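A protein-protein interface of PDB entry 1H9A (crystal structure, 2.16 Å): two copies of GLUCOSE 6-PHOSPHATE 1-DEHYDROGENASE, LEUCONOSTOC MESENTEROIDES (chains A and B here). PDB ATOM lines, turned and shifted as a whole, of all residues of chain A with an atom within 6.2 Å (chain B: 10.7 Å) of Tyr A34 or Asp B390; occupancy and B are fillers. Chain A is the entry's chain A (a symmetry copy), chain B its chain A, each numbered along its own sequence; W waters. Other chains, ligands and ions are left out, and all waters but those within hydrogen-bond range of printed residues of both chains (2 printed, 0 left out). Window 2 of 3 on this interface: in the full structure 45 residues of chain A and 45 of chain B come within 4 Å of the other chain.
The side-chain carboxylate (OD1) of Asp B390 is in salt-bridge range of the side-chain amino group (NZ) of Lys A32, 3.2 Å away. OD2 of Asp B390 sits at hydrogen-bond distance from OH of Tyr A34, 2.8 Å away.
The guanidinium group (NH1) of Arg A417 lies close to the backbone carbonyl oxygen (O) of Pro A412. The side-chain carboxylate (OE2) of Glu A416 lies within salt-bridge range of the side-chain amino group (NZ) of Lys A32, at 2.9 Å. The backbone carbonyl oxygen (O) of Leu A29 lies within hydrogen-bond range of the backbone NH (N) of Tyr A34 (2.9 Å). The backbone carbonyl oxygen of Tyr A34 sits at hydrogen-bond distance from the backbone NH of Ile A4.
C of Asn A410 touches CG1 of Val B388, at 3.7 Å. OD1 of Asp B390 touches CG of Pro A412, at 3.7 Å.
No residue of chain B comes within 4 Å of Ile A4. No residue of chain B comes within 4 Å of Leu A29. No residue of chain B comes within 4 Å of Gly A33. Of chain B, only Asp B390 comes within 4 Å of Tyr A34. Of the printed residues of chain B, Asn A410 touches Val B388. Of the printed residues of chain B, Pro A412 touches Asp B390 (3.7 Å). Of the printed residues of chain A, Val B388 touches Asn A410 (3.7 Å). Asp B390 touches just these residues of chain A: Lys A32 (3.2 Å), Tyr A34 (2.8 Å) and Pro A412 (3.7 Å). The nearest residue of chain B that does not touch Tyr A34 is Ala B391 (5.3 Å).
Of the 20 printed residues of chain A, 4 touch a printed residue of chain B. Hydrophobic or aromatic side chains of chain A that line the printed part of chain B: Tyr A34 and Pro A412. Of the 11 printed residues of chain B, 2 touch a printed residue of chain A. Hydrophobic or aromatic side chains of chain B that line the printed part of chain A: Val B388.
No position is printed for both chains.
Water W2 lies within hydrogen-bond range of a ring nitrogen (ND1) of His A420, the side-chain carboxylate of Glu A416 and the side-chain carboxylate of Asp B390. Water W1 lies within hydrogen-bond range of O of Glu B389, NE of Arg A417 and O of Asp B390.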
ATOM      1  N   VAL A   1      -7.926  31.919  14.249  1.00  0.00           N
ATOM      2  CA  VAL A   1      -9.026  30.951  13.954  1.00  0.00           C
ATOM      3  C   VAL A   1      -9.024  29.947  15.099  1.00  0.00           C
ATOM      4  O   VAL A   1      -7.966  29.696  15.676  1.00  0.00           O
ATOM      5  CB  VAL A   1      -8.779  30.185  12.633  1.00  0.00           C
ATOM      6  CG1 VAL A   1     -10.052  29.500  12.205  1.00  0.00           C
ATOM      7  CG2 VAL A   1      -8.276  31.127  11.539  1.00  0.00           C
ATOM      8  N   SER A   2     -10.182  29.380  15.428  1.00  0.00           N
ATOM      9  CA  SER A   2     -10.282  28.418  16.530  1.00  0.00           C
ATOM     10  C   SER A   2      -9.718  27.024  16.179  1.00  0.00           C
ATOM     11  O   SER A   2      -9.885  26.545  15.053  1.00  0.00           O
ATOM     12  CB  SER A   2     -11.740  28.321  16.997  1.00  0.00           C
ATOM     13  OG  SER A   2     -11.847  27.573  18.195  1.00  0.00           O
ATOM     14  N   GLU A   3      -9.078  26.380  17.156  1.00  0.00           N
ATOM     15  CA  GLU A   3      -8.465  25.060  16.978  1.00  0.00           C
ATOM     16  C   GLU A   3      -9.406  23.850  17.033  1.00  0.00           C
ATOM     17  O   GLU A   3     -10.241  23.724  17.935  1.00  0.00           O
ATOM     18  CB  GLU A   3      -7.338  24.854  18.006  1.00  0.00           C
ATOM     19  CG  GLU A   3      -6.723  23.455  17.977  1.00  0.00           C
ATOM     20  CD  GLU A   3      -5.759  23.179  19.121  1.00  0.00           C
ATOM     21  OE1 GLU A   3      -5.996  23.664  20.250  1.00  0.00           O
ATOM     22  OE2 GLU A   3      -4.766  22.456  18.892  1.00  0.00           O
ATOM     23  N   ILE A   4      -9.219  22.940  16.080  1.00  0.00           N
ATOM     24  CA  ILE A   4      -9.990  21.703  15.995  1.00  0.00           C
ATOM     25  C   ILE A   4      -9.142  20.583  16.621  1.00  0.00           C
ATOM     26  O   ILE A   4      -8.028  20.302  16.171  1.00  0.00           O
ATOM     27  CB  ILE A   4     -10.310  21.334  14.515  1.00  0.00           C
ATOM     28  CG1 ILE A   4     -11.198  22.401  13.874  1.00  0.00           C
ATOM     29  CG2 ILE A   4     -10.997  19.978  14.437  1.00  0.00           C
ATOM     30  CD1 ILE A   4     -11.463  22.165  12.400  1.00  0.00           C
ATOM     31  N   LYS A   5      -9.644  19.993  17.699  1.00  0.00           N
ATOM     32  CA  LYS A   5      -8.945  18.909  18.384  1.00  0.00           C
ATOM     33  C   LYS A   5      -9.561  17.611  17.880  1.00  0.00           C
ATOM     34  O   LYS A   5     -10.715  17.300  18.199  1.00  0.00           O
ATOM     35  CB  LYS A   5      -9.137  19.042  19.894  1.00  0.00           C
ATOM     36  CG  LYS A   5      -8.715  20.394  20.451  1.00  0.00           C
ATOM     37  CD  LYS A   5      -8.876  20.435  21.961  1.00  0.00           C
ATOM     38  CE  LYS A   5      -8.233  21.677  22.570  1.00  0.00           C
ATOM     39  NZ  LYS A   5      -8.005  21.506  24.044  1.00  0.00           N
ATOM     40  N   ASN A  28      -3.899  21.509   4.155  1.00  0.00           N
ATOM     41  CA  ASN A  28      -4.513  22.817   3.934  1.00  0.00           C
ATOM     42  C   ASN A  28      -5.198  23.352   5.186  1.00  0.00           C
ATOM     43  O   ASN A  28      -5.121  24.544   5.491  1.00  0.00           O
ATOM     44  CB  ASN A  28      -5.529  22.740   2.793  1.00  0.00           C
ATOM     45  CG  ASN A  28      -5.150  23.613   1.625  1.00  0.00           C
ATOM     46  OD1 ASN A  28      -4.171  23.341   0.930  1.00  0.00           O
ATOM     47  ND2 ASN A  28      -5.914  24.682   1.408  1.00  0.00           N
ATOM     48  N   LEU A  29      -5.882  22.467   5.902  1.00  0.00           N
ATOM     49  CA  LEU A  29      -6.566  22.844   7.128  1.00  0.00           C
ATOM     50  C   LEU A  29      -5.546  23.267   8.182  1.00  0.00           C
ATOM     51  O   LEU A  29      -5.861  24.052   9.081  1.00  0.00           O
ATOM     52  CB  LEU A  29      -7.407  21.677   7.642  1.00  0.00           C
ATOM     53  CG  LEU A  29      -8.619  21.308   6.784  1.00  0.00           C
ATOM     54  CD1 LEU A  29      -9.310  20.103   7.378  1.00  0.00           C
ATOM     55  CD2 LEU A  29      -9.580  22.483   6.704  1.00  0.00           C
ATOM     56  N   TYR A  30      -4.335  22.722   8.083  1.00  0.00           N
ATOM     57  CA  TYR A  30      -3.259  23.046   9.009  1.00  0.00           C
ATOM     58  C   TYR A  30      -2.685  24.408   8.627  1.00  0.00           C
ATOM     59  O   TYR A  30      -2.422  25.240   9.489  1.00  0.00           O
ATOM     60  CB  TYR A  30      -2.177  21.959   8.958  1.00  0.00           C
ATOM     61  CG  TYR A  30      -0.959  22.229   9.820  1.00  0.00           C
ATOM     62  CD1 TYR A  30      -0.950  21.902  11.183  1.00  0.00           C
ATOM     63  CD2 TYR A  30       0.181  22.826   9.277  1.00  0.00           C
ATOM     64  CE1 TYR A  30       0.171  22.170  11.985  1.00  0.00           C
ATOM     65  CE2 TYR A  30       1.308  23.095  10.071  1.00  0.00           C
ATOM     66  CZ  TYR A  30       1.290  22.766  11.416  1.00  0.00           C
ATOM     67  OH  TYR A  30       2.394  23.040  12.182  1.00  0.00           O
ATOM     68  N   LYS A  31      -2.520  24.644   7.328  1.00  0.00           N
ATOM     69  CA  LYS A  31      -1.990  25.914   6.842  1.00  0.00           C
ATOM     70  C   LYS A  31      -2.889  27.077   7.245  1.00  0.00           C
ATOM     71  O   LYS A  31      -2.409  28.169   7.544  1.00  0.00           O
ATOM     72  CB  LYS A  31      -1.819  25.887   5.321  1.00  0.00           C
ATOM     73  CG  LYS A  31      -0.710  24.963   4.864  1.00  0.00           C
ATOM     74  CD  LYS A  31      -0.109  25.416   3.547  1.00  0.00           C
ATOM     75  CE  LYS A  31      -0.703  24.670   2.372  1.00  0.00           C
ATOM     76  NZ  LYS A  31      -0.024  25.077   1.111  1.00  0.00           N
ATOM     77  N   LYS A  32      -4.195  26.822   7.268  1.00  0.00           N
ATOM     78  CA  LYS A  32      -5.186  27.826   7.639  1.00  0.00           C
ATOM     79  C   LYS A  32      -5.307  27.999   9.162  1.00  0.00           C
ATOM     80  O   LYS A  32      -6.072  28.844   9.645  1.00  0.00           O
ATOM     81  CB  LYS A  32      -6.544  27.469   7.021  1.00  0.00           C
ATOM     82  CG  LYS A  32      -6.530  27.453   5.500  1.00  0.00           C
ATOM     83  CD  LYS A  32      -7.883  27.103   4.913  1.00  0.00           C
ATOM     84  CE  LYS A  32      -7.857  27.263   3.399  1.00  0.00           C
ATOM     85  NZ  LYS A  32      -9.218  27.169   2.792  1.00  0.00           N
ATOM     86  N   GLY A  33      -4.574  27.181   9.912  1.00  0.00           N
ATOM     87  CA  GLY A  33      -4.600  27.279  11.360  1.00  0.00           C
ATOM     88  C   GLY A  33      -5.717  26.560  12.089  1.00  0.00           C
ATOM     89  O   GLY A  33      -5.900  26.769  13.287  1.00  0.00           O
ATOM     90  N   TYR A  34      -6.482  25.731  11.392  1.00  0.00           N
ATOM     91  CA  TYR A  34      -7.556  24.997  12.052  1.00  0.00           C
ATOM     92  C   TYR A  34      -6.958  23.877  12.896  1.00  0.00           C
ATOM     93  O   TYR A  34      -7.398  23.628  14.022  1.00  0.00           O
ATOM     94  CB  TYR A  34      -8.533  24.432  11.027  1.00  0.00           C
ATOM     95  CG  TYR A  34      -9.404  25.492  10.408  1.00  0.00           C
ATOM     96  CD1 TYR A  34     -10.438  26.076  11.137  1.00  0.00           C
ATOM     97  CD2 TYR A  34      -9.184  25.928   9.101  1.00  0.00           C
ATOM     98  CE1 TYR A  34     -11.234  27.070  10.585  1.00  0.00           C
ATOM     99  CE2 TYR A  34      -9.973  26.925   8.537  1.00  0.00           C
ATOM    100  CZ  TYR A  34     -11.000  27.492   9.288  1.00  0.00           C
ATOM    101  OH  TYR A  34     -11.799  28.471   8.743  1.00  0.00           O
ATOM    102  N   LEU A  35      -5.939  23.222  12.348  1.00  0.00           N
ATOM    103  CA  LEU A  35      -5.250  22.136  13.036  1.00  0.00           C
ATOM    104  C   LEU A  35      -3.950  22.706  13.588  1.00  0.00           C
ATOM    105  O   LEU A  35      -3.124  23.219  12.832  1.00  0.00           O
ATOM    106  CB  LEU A  35      -4.949  21.009  12.053  1.00  0.00           C
ATOM    107  CG  LEU A  35      -6.159  20.360  11.380  1.00  0.00           C
ATOM    108  CD1 LEU A  35      -5.688  19.419  10.289  1.00  0.00           C
ATOM    109  CD2 LEU A  35      -6.999  19.634  12.407  1.00  0.00           C
ATOM    110  N   GLN A  36      -3.771  22.638  14.901  1.00  0.00           N
ATOM    111  CA  GLN A  36      -2.566  23.184  15.517  1.00  0.00           C
ATOM    112  C   GLN A  36      -1.720  22.182  16.295  1.00  0.00           C
ATOM    113  O   GLN A  36      -0.846  21.536  15.730  1.00  0.00           O
ATOM    114  CB  GLN A  36      -2.927  24.370  16.414  1.00  0.00           C
ATOM    115  CG  GLN A  36      -3.590  25.533  15.696  1.00  0.00           C
ATOM    116  CD  GLN A  36      -4.394  26.405  16.643  1.00  0.00           C
ATOM    117  OE1 GLN A  36      -4.106  26.469  17.844  1.00  0.00           O
ATOM    118  NE2 GLN A  36      -5.428  27.055  16.120  1.00  0.00           N
ATOM    119  N   ASN A 410      -9.478  31.274  -3.542  1.00  0.00           N
ATOM    120  CA  ASN A 410      -9.931  31.032  -2.162  1.00  0.00           C
ATOM    121  C   ASN A 410     -10.882  29.860  -1.951  1.00  0.00           C
ATOM    122  O   ASN A 410     -11.160  29.485  -0.803  1.00  0.00           O
ATOM    123  CB  ASN A 410     -10.594  32.283  -1.580  1.00  0.00           C
ATOM    124  CG  ASN A 410      -9.629  33.434  -1.406  1.00  0.00           C
ATOM    125  OD1 ASN A 410      -8.410  33.261  -1.482  1.00  0.00           O
ATOM    126  ND2 ASN A 410     -10.168  34.622  -1.169  1.00  0.00           N
ATOM    127  N   PRO A 412     -12.113  26.296  -1.428  1.00  0.00           N
ATOM    128  CA  PRO A 412     -11.535  25.041  -0.924  1.00  0.00           C
ATOM    129  C   PRO A 412     -11.859  23.889  -1.876  1.00  0.00           C
ATOM    130  O   PRO A 412     -12.912  23.903  -2.521  1.00  0.00           O
ATOM    131  CB  PRO A 412     -12.269  24.839   0.405  1.00  0.00           C
ATOM    132  CG  PRO A 412     -12.679  26.238   0.807  1.00  0.00           C
ATOM    133  CD  PRO A 412     -13.124  26.820  -0.494  1.00  0.00           C
ATOM    134  N   GLU A 416     -11.350  19.007   0.961  1.00  0.00           N
ATOM    135  CA  GLU A 416     -10.982  19.816   2.118  1.00  0.00           C
ATOM    136  C   GLU A 416     -12.270  20.181   2.853  1.00  0.00           C
ATOM    137  O   GLU A 416     -12.392  20.001   4.069  1.00  0.00           O
ATOM    138  CB  GLU A 416     -10.284  21.101   1.666  1.00  0.00           C
ATOM    139  CG  GLU A 416      -9.821  21.975   2.823  1.00  0.00           C
ATOM    140  CD  GLU A 416      -9.344  23.356   2.394  1.00  0.00           C
ATOM    141  OE1 GLU A 416      -8.611  23.480   1.386  1.00  0.00           O
ATOM    142  OE2 GLU A 416      -9.706  24.330   3.087  1.00  0.00           O
ATOM    143  N   ARG A 417     -13.237  20.672   2.085  1.00  0.00           N
ATOM    144  CA  ARG A 417     -14.535  21.077   2.602  1.00  0.00           C
ATOM    145  C   ARG A 417     -15.230  19.949   3.353  1.00  0.00           C
ATOM    146  O   ARG A 417     -15.703  20.148   4.475  1.00  0.00           O
ATOM    147  CB  ARG A 417     -15.434  21.557   1.458  1.00  0.00           C
ATOM    148  CG  ARG A 417     -16.838  21.959   1.907  1.00  0.00           C
ATOM    149  CD  ARG A 417     -16.956  23.454   2.135  1.00  0.00           C
ATOM    150  NE  ARG A 417     -17.467  24.127   0.940  1.00  0.00           N
ATOM    151  CZ  ARG A 417     -16.741  24.476  -0.124  1.00  0.00           C
ATOM    152  NH1 ARG A 417     -15.436  24.231  -0.174  1.00  0.00           N
ATOM    153  NH2 ARG A 417     -17.332  25.046  -1.166  1.00  0.00           N
ATOM    154  N   HIS A 420     -13.400  19.006   6.560  1.00  0.00           N
ATOM    155  CA  HIS A 420     -13.603  20.114   7.489  1.00  0.00           C
ATOM    156  C   HIS A 420     -15.026  20.097   8.077  1.00  0.00           C
ATOM    157  O   HIS A 420     -15.205  20.276   9.289  1.00  0.00           O
ATOM    158  CB  HIS A 420     -13.321  21.437   6.775  1.00  0.00           C
ATOM    159  CG  HIS A 420     -13.181  22.608   7.701  1.00  0.00           C
ATOM    160  ND1 HIS A 420     -12.850  23.865   7.246  1.00  0.00           N
ATOM    161  CD2 HIS A 420     -13.341  22.723   9.037  1.00  0.00           C
ATOM    162  CE1 HIS A 420     -12.813  24.705   8.264  1.00  0.00           C
ATOM    163  NE2 HIS A 420     -13.109  24.035   9.363  1.00  0.00           N
ATOM    164  N   ASP A 421     -16.027  19.856   7.232  1.00  0.00           N
ATOM    165  CA  ASP A 421     -17.412  19.798   7.692  1.00  0.00           C
ATOM    166  C   ASP A 421     -17.601  18.658   8.680  1.00  0.00           C
ATOM    167  O   ASP A 421     -18.338  18.802   9.658  1.00  0.00           O
ATOM    168  CB  ASP A 421     -18.380  19.648   6.516  1.00  0.00           C
ATOM    169  CG  ASP A 421     -18.610  20.960   5.770  1.00  0.00           C
ATOM    170  OD1 ASP A 421     -18.003  21.990   6.132  1.00  0.00           O
ATOM    171  OD2 ASP A 421     -19.407  20.964   4.811  1.00  0.00           O
ATOM    172  N   SER B 360     -25.184  33.171  10.010  1.00  0.00           N
ATOM    173  CA  SER B 360     -23.885  33.651   9.544  1.00  0.00           C
ATOM    174  C   SER B 360     -23.520  34.979  10.191  1.00  0.00           C
ATOM    175  O   SER B 360     -24.375  35.633  10.802  1.00  0.00           O
ATOM    176  CB  SER B 360     -23.912  33.815   8.016  1.00  0.00           C
ATOM    177  OG  SER B 360     -25.068  34.531   7.590  1.00  0.00           O
ATOM    178  N   GLU B 361     -22.255  35.379  10.046  1.00  0.00           N
ATOM    179  CA  GLU B 361     -21.777  36.649  10.601  1.00  0.00           C
ATOM    180  C   GLU B 361     -22.434  37.800   9.823  1.00  0.00           C
ATOM    181  O   GLU B 361     -22.963  38.747  10.413  1.00  0.00           O
ATOM    182  CB  GLU B 361     -20.241  36.733  10.518  1.00  0.00           C
ATOM    183  CG  GLU B 361     -19.618  37.913  11.291  1.00  0.00           C
ATOM    184  CD  GLU B 361     -18.151  37.677  11.663  1.00  0.00           C
ATOM    185  OE1 GLU B 361     -17.890  37.040  12.714  1.00  0.00           O
ATOM    186  OE2 GLU B 361     -17.258  38.132  10.908  1.00  0.00           O
ATOM    187  N   LYS B 386     -23.482  33.230  -1.694  1.00  0.00           N
ATOM    188  CA  LYS B 386     -22.586  32.704  -0.662  1.00  0.00           C
ATOM    189  C   LYS B 386     -21.178  33.259  -0.866  1.00  0.00           C
ATOM    190  O   LYS B 386     -20.696  33.337  -2.000  1.00  0.00           O
ATOM    191  CB  LYS B 386     -22.556  31.168  -0.695  1.00  0.00           C
ATOM    192  CG  LYS B 386     -21.664  30.535   0.364  1.00  0.00           C
ATOM    193  CD  LYS B 386     -21.489  29.044   0.125  1.00  0.00           C
ATOM    194  CE  LYS B 386     -20.595  28.403   1.185  1.00  0.00           C
ATOM    195  NZ  LYS B 386     -19.186  28.915   1.178  1.00  0.00           N
ATOM    196  N   SER B 387     -20.543  33.689   0.221  1.00  0.00           N
ATOM    197  CA  SER B 387     -19.185  34.219   0.161  1.00  0.00           C
ATOM    198  C   SER B 387     -18.214  33.055   0.024  1.00  0.00           C
ATOM    199  O   SER B 387     -18.552  31.918   0.351  1.00  0.00           O
ATOM    200  CB  SER B 387     -18.858  35.003   1.432  1.00  0.00           C
ATOM    201  OG  SER B 387     -18.876  34.154   2.562  1.00  0.00           O
ATOM    202  N   VAL B 388     -17.022  33.333  -0.486  1.00  0.00           N
ATOM    203  CA  VAL B 388     -16.019  32.291  -0.639  1.00  0.00           C
ATOM    204  C   VAL B 388     -15.215  32.229   0.657  1.00  0.00           C
ATOM    205  O   VAL B 388     -14.122  32.791   0.755  1.00  0.00           O
ATOM    206  CB  VAL B 388     -15.065  32.566  -1.821  1.00  0.00           C
ATOM    207  CG1 VAL B 388     -14.217  31.339  -2.087  1.00  0.00           C
ATOM    208  CG2 VAL B 388     -15.854  32.950  -3.070  1.00  0.00           C
ATOM    209  N   GLU B 389     -15.814  31.630   1.678  1.00  0.00           N
ATOM    210  CA  GLU B 389     -15.173  31.484   2.975  1.00  0.00           C
ATOM    211  C   GLU B 389     -15.386  30.050   3.417  1.00  0.00           C
ATOM    212  O   GLU B 389     -16.166  29.313   2.804  1.00  0.00           O
ATOM    213  CB  GLU B 389     -15.779  32.451   3.992  1.00  0.00           C
ATOM    214  CG  GLU B 389     -15.470  33.902   3.691  1.00  0.00           C
ATOM    215  CD  GLU B 389     -16.084  34.863   4.689  1.00  0.00           C
ATOM    216  OE1 GLU B 389     -17.317  35.038   4.665  1.00  0.00           O
ATOM    217  OE2 GLU B 389     -15.329  35.460   5.492  1.00  0.00           O
ATOM    218  N   ASP B 390     -14.657  29.637   4.449  1.00  0.00           N
ATOM    219  CA  ASP B 390     -14.778  28.275   4.961  1.00  0.00           C
ATOM    220  C   ASP B 390     -16.136  28.130   5.654  1.00  0.00           C
ATOM    221  O   ASP B 390     -16.844  27.143   5.457  1.00  0.00           O
ATOM    222  CB  ASP B 390     -13.619  27.952   5.919  1.00  0.00           C
ATOM    223  CG  ASP B 390     -12.244  28.208   5.294  1.00  0.00           C
ATOM    224  OD1 ASP B 390     -12.008  27.779   4.144  1.00  0.00           O
ATOM    225  OD2 ASP B 390     -11.395  28.849   5.953  1.00  0.00           O
ATOM    226  N   ALA B 391     -16.501  29.124   6.455  1.00  0.00           N
ATOM    227  CA  ALA B 391     -17.781  29.102   7.143  1.00  0.00           C
ATOM    228  C   ALA B 391     -18.817  29.705   6.204  1.00  0.00           C
ATOM    229  O   ALA B 391     -18.500  30.604   5.420  1.00  0.00           O
ATOM    230  CB  ALA B 391     -17.704  29.906   8.434  1.00  0.00           C
ATOM    231  N   PHE B 392     -20.047  29.211   6.278  1.00  0.00           N
ATOM    232  CA  PHE B 392     -21.111  29.719   5.425  1.00  0.00           C
ATOM    233  C   PHE B 392     -21.411  31.165   5.805  1.00  0.00           C
ATOM    234  O   PHE B 392     -21.620  31.483   6.981  1.00  0.00           O
ATOM    235  CB  PHE B 392     -22.381  28.871   5.551  1.00  0.00           C
ATOM    236  CG  PHE B 392     -23.436  29.213   4.532  1.00  0.00           C
ATOM    237  CD1 PHE B 392     -24.269  30.314   4.711  1.00  0.00           C
ATOM    238  CD2 PHE B 392     -23.567  28.457   3.369  1.00  0.00           C
ATOM    239  CE1 PHE B 392     -25.211  30.659   3.749  1.00  0.00           C
ATOM    240  CE2 PHE B 392     -24.510  28.794   2.399  1.00  0.00           C
ATOM    241  CZ  PHE B 392     -25.331  29.898   2.590  1.00  0.00           C
ATOM    242  N   ASN B 393     -21.463  32.024   4.796  1.00  0.00           N
ATOM    243  CA  ASN B 393     -21.720  33.440   4.996  1.00  0.00           C
ATOM    244  C   ASN B 393     -22.242  33.995   3.678  1.00  0.00           C
ATOM    245  O   ASN B 393     -22.069  33.360   2.631  1.00  0.00           O
ATOM    246  CB  ASN B 393     -20.411  34.134   5.376  1.00  0.00           C
ATOM    247  CG  ASN B 393     -20.624  35.507   5.956  1.00  0.00           C
ATOM    248  OD1 ASN B 393     -21.551  35.721   6.732  1.00  0.00           O
ATOM    249  ND2 ASN B 393     -19.749  36.443   5.610  1.00  0.00           N
ATOM    250  N   THR B 394     -22.883  35.162   3.721  1.00  0.00           N
ATOM    251  CA  THR B 394     -23.428  35.790   2.519  1.00  0.00           C
ATOM    252  C   THR B 394     -22.589  36.975   2.043  1.00  0.00           C
ATOM    253  O   THR B 394     -21.788  37.530   2.800  1.00  0.00           O
ATOM    254  CB  THR B 394     -24.897  36.260   2.728  1.00  0.00           C
ATOM    255  OG1 THR B 394     -24.952  37.259   3.754  1.00  0.00           O
ATOM    256  CG2 THR B 394     -25.782  35.091   3.119  1.00  0.00           C
HETATM  257  O   HOH W   1     -16.422  26.519   2.183  1.00  0.00           O
HETATM  258  O   HOH W   2     -11.721  24.604   5.043  1.00  0.00           O
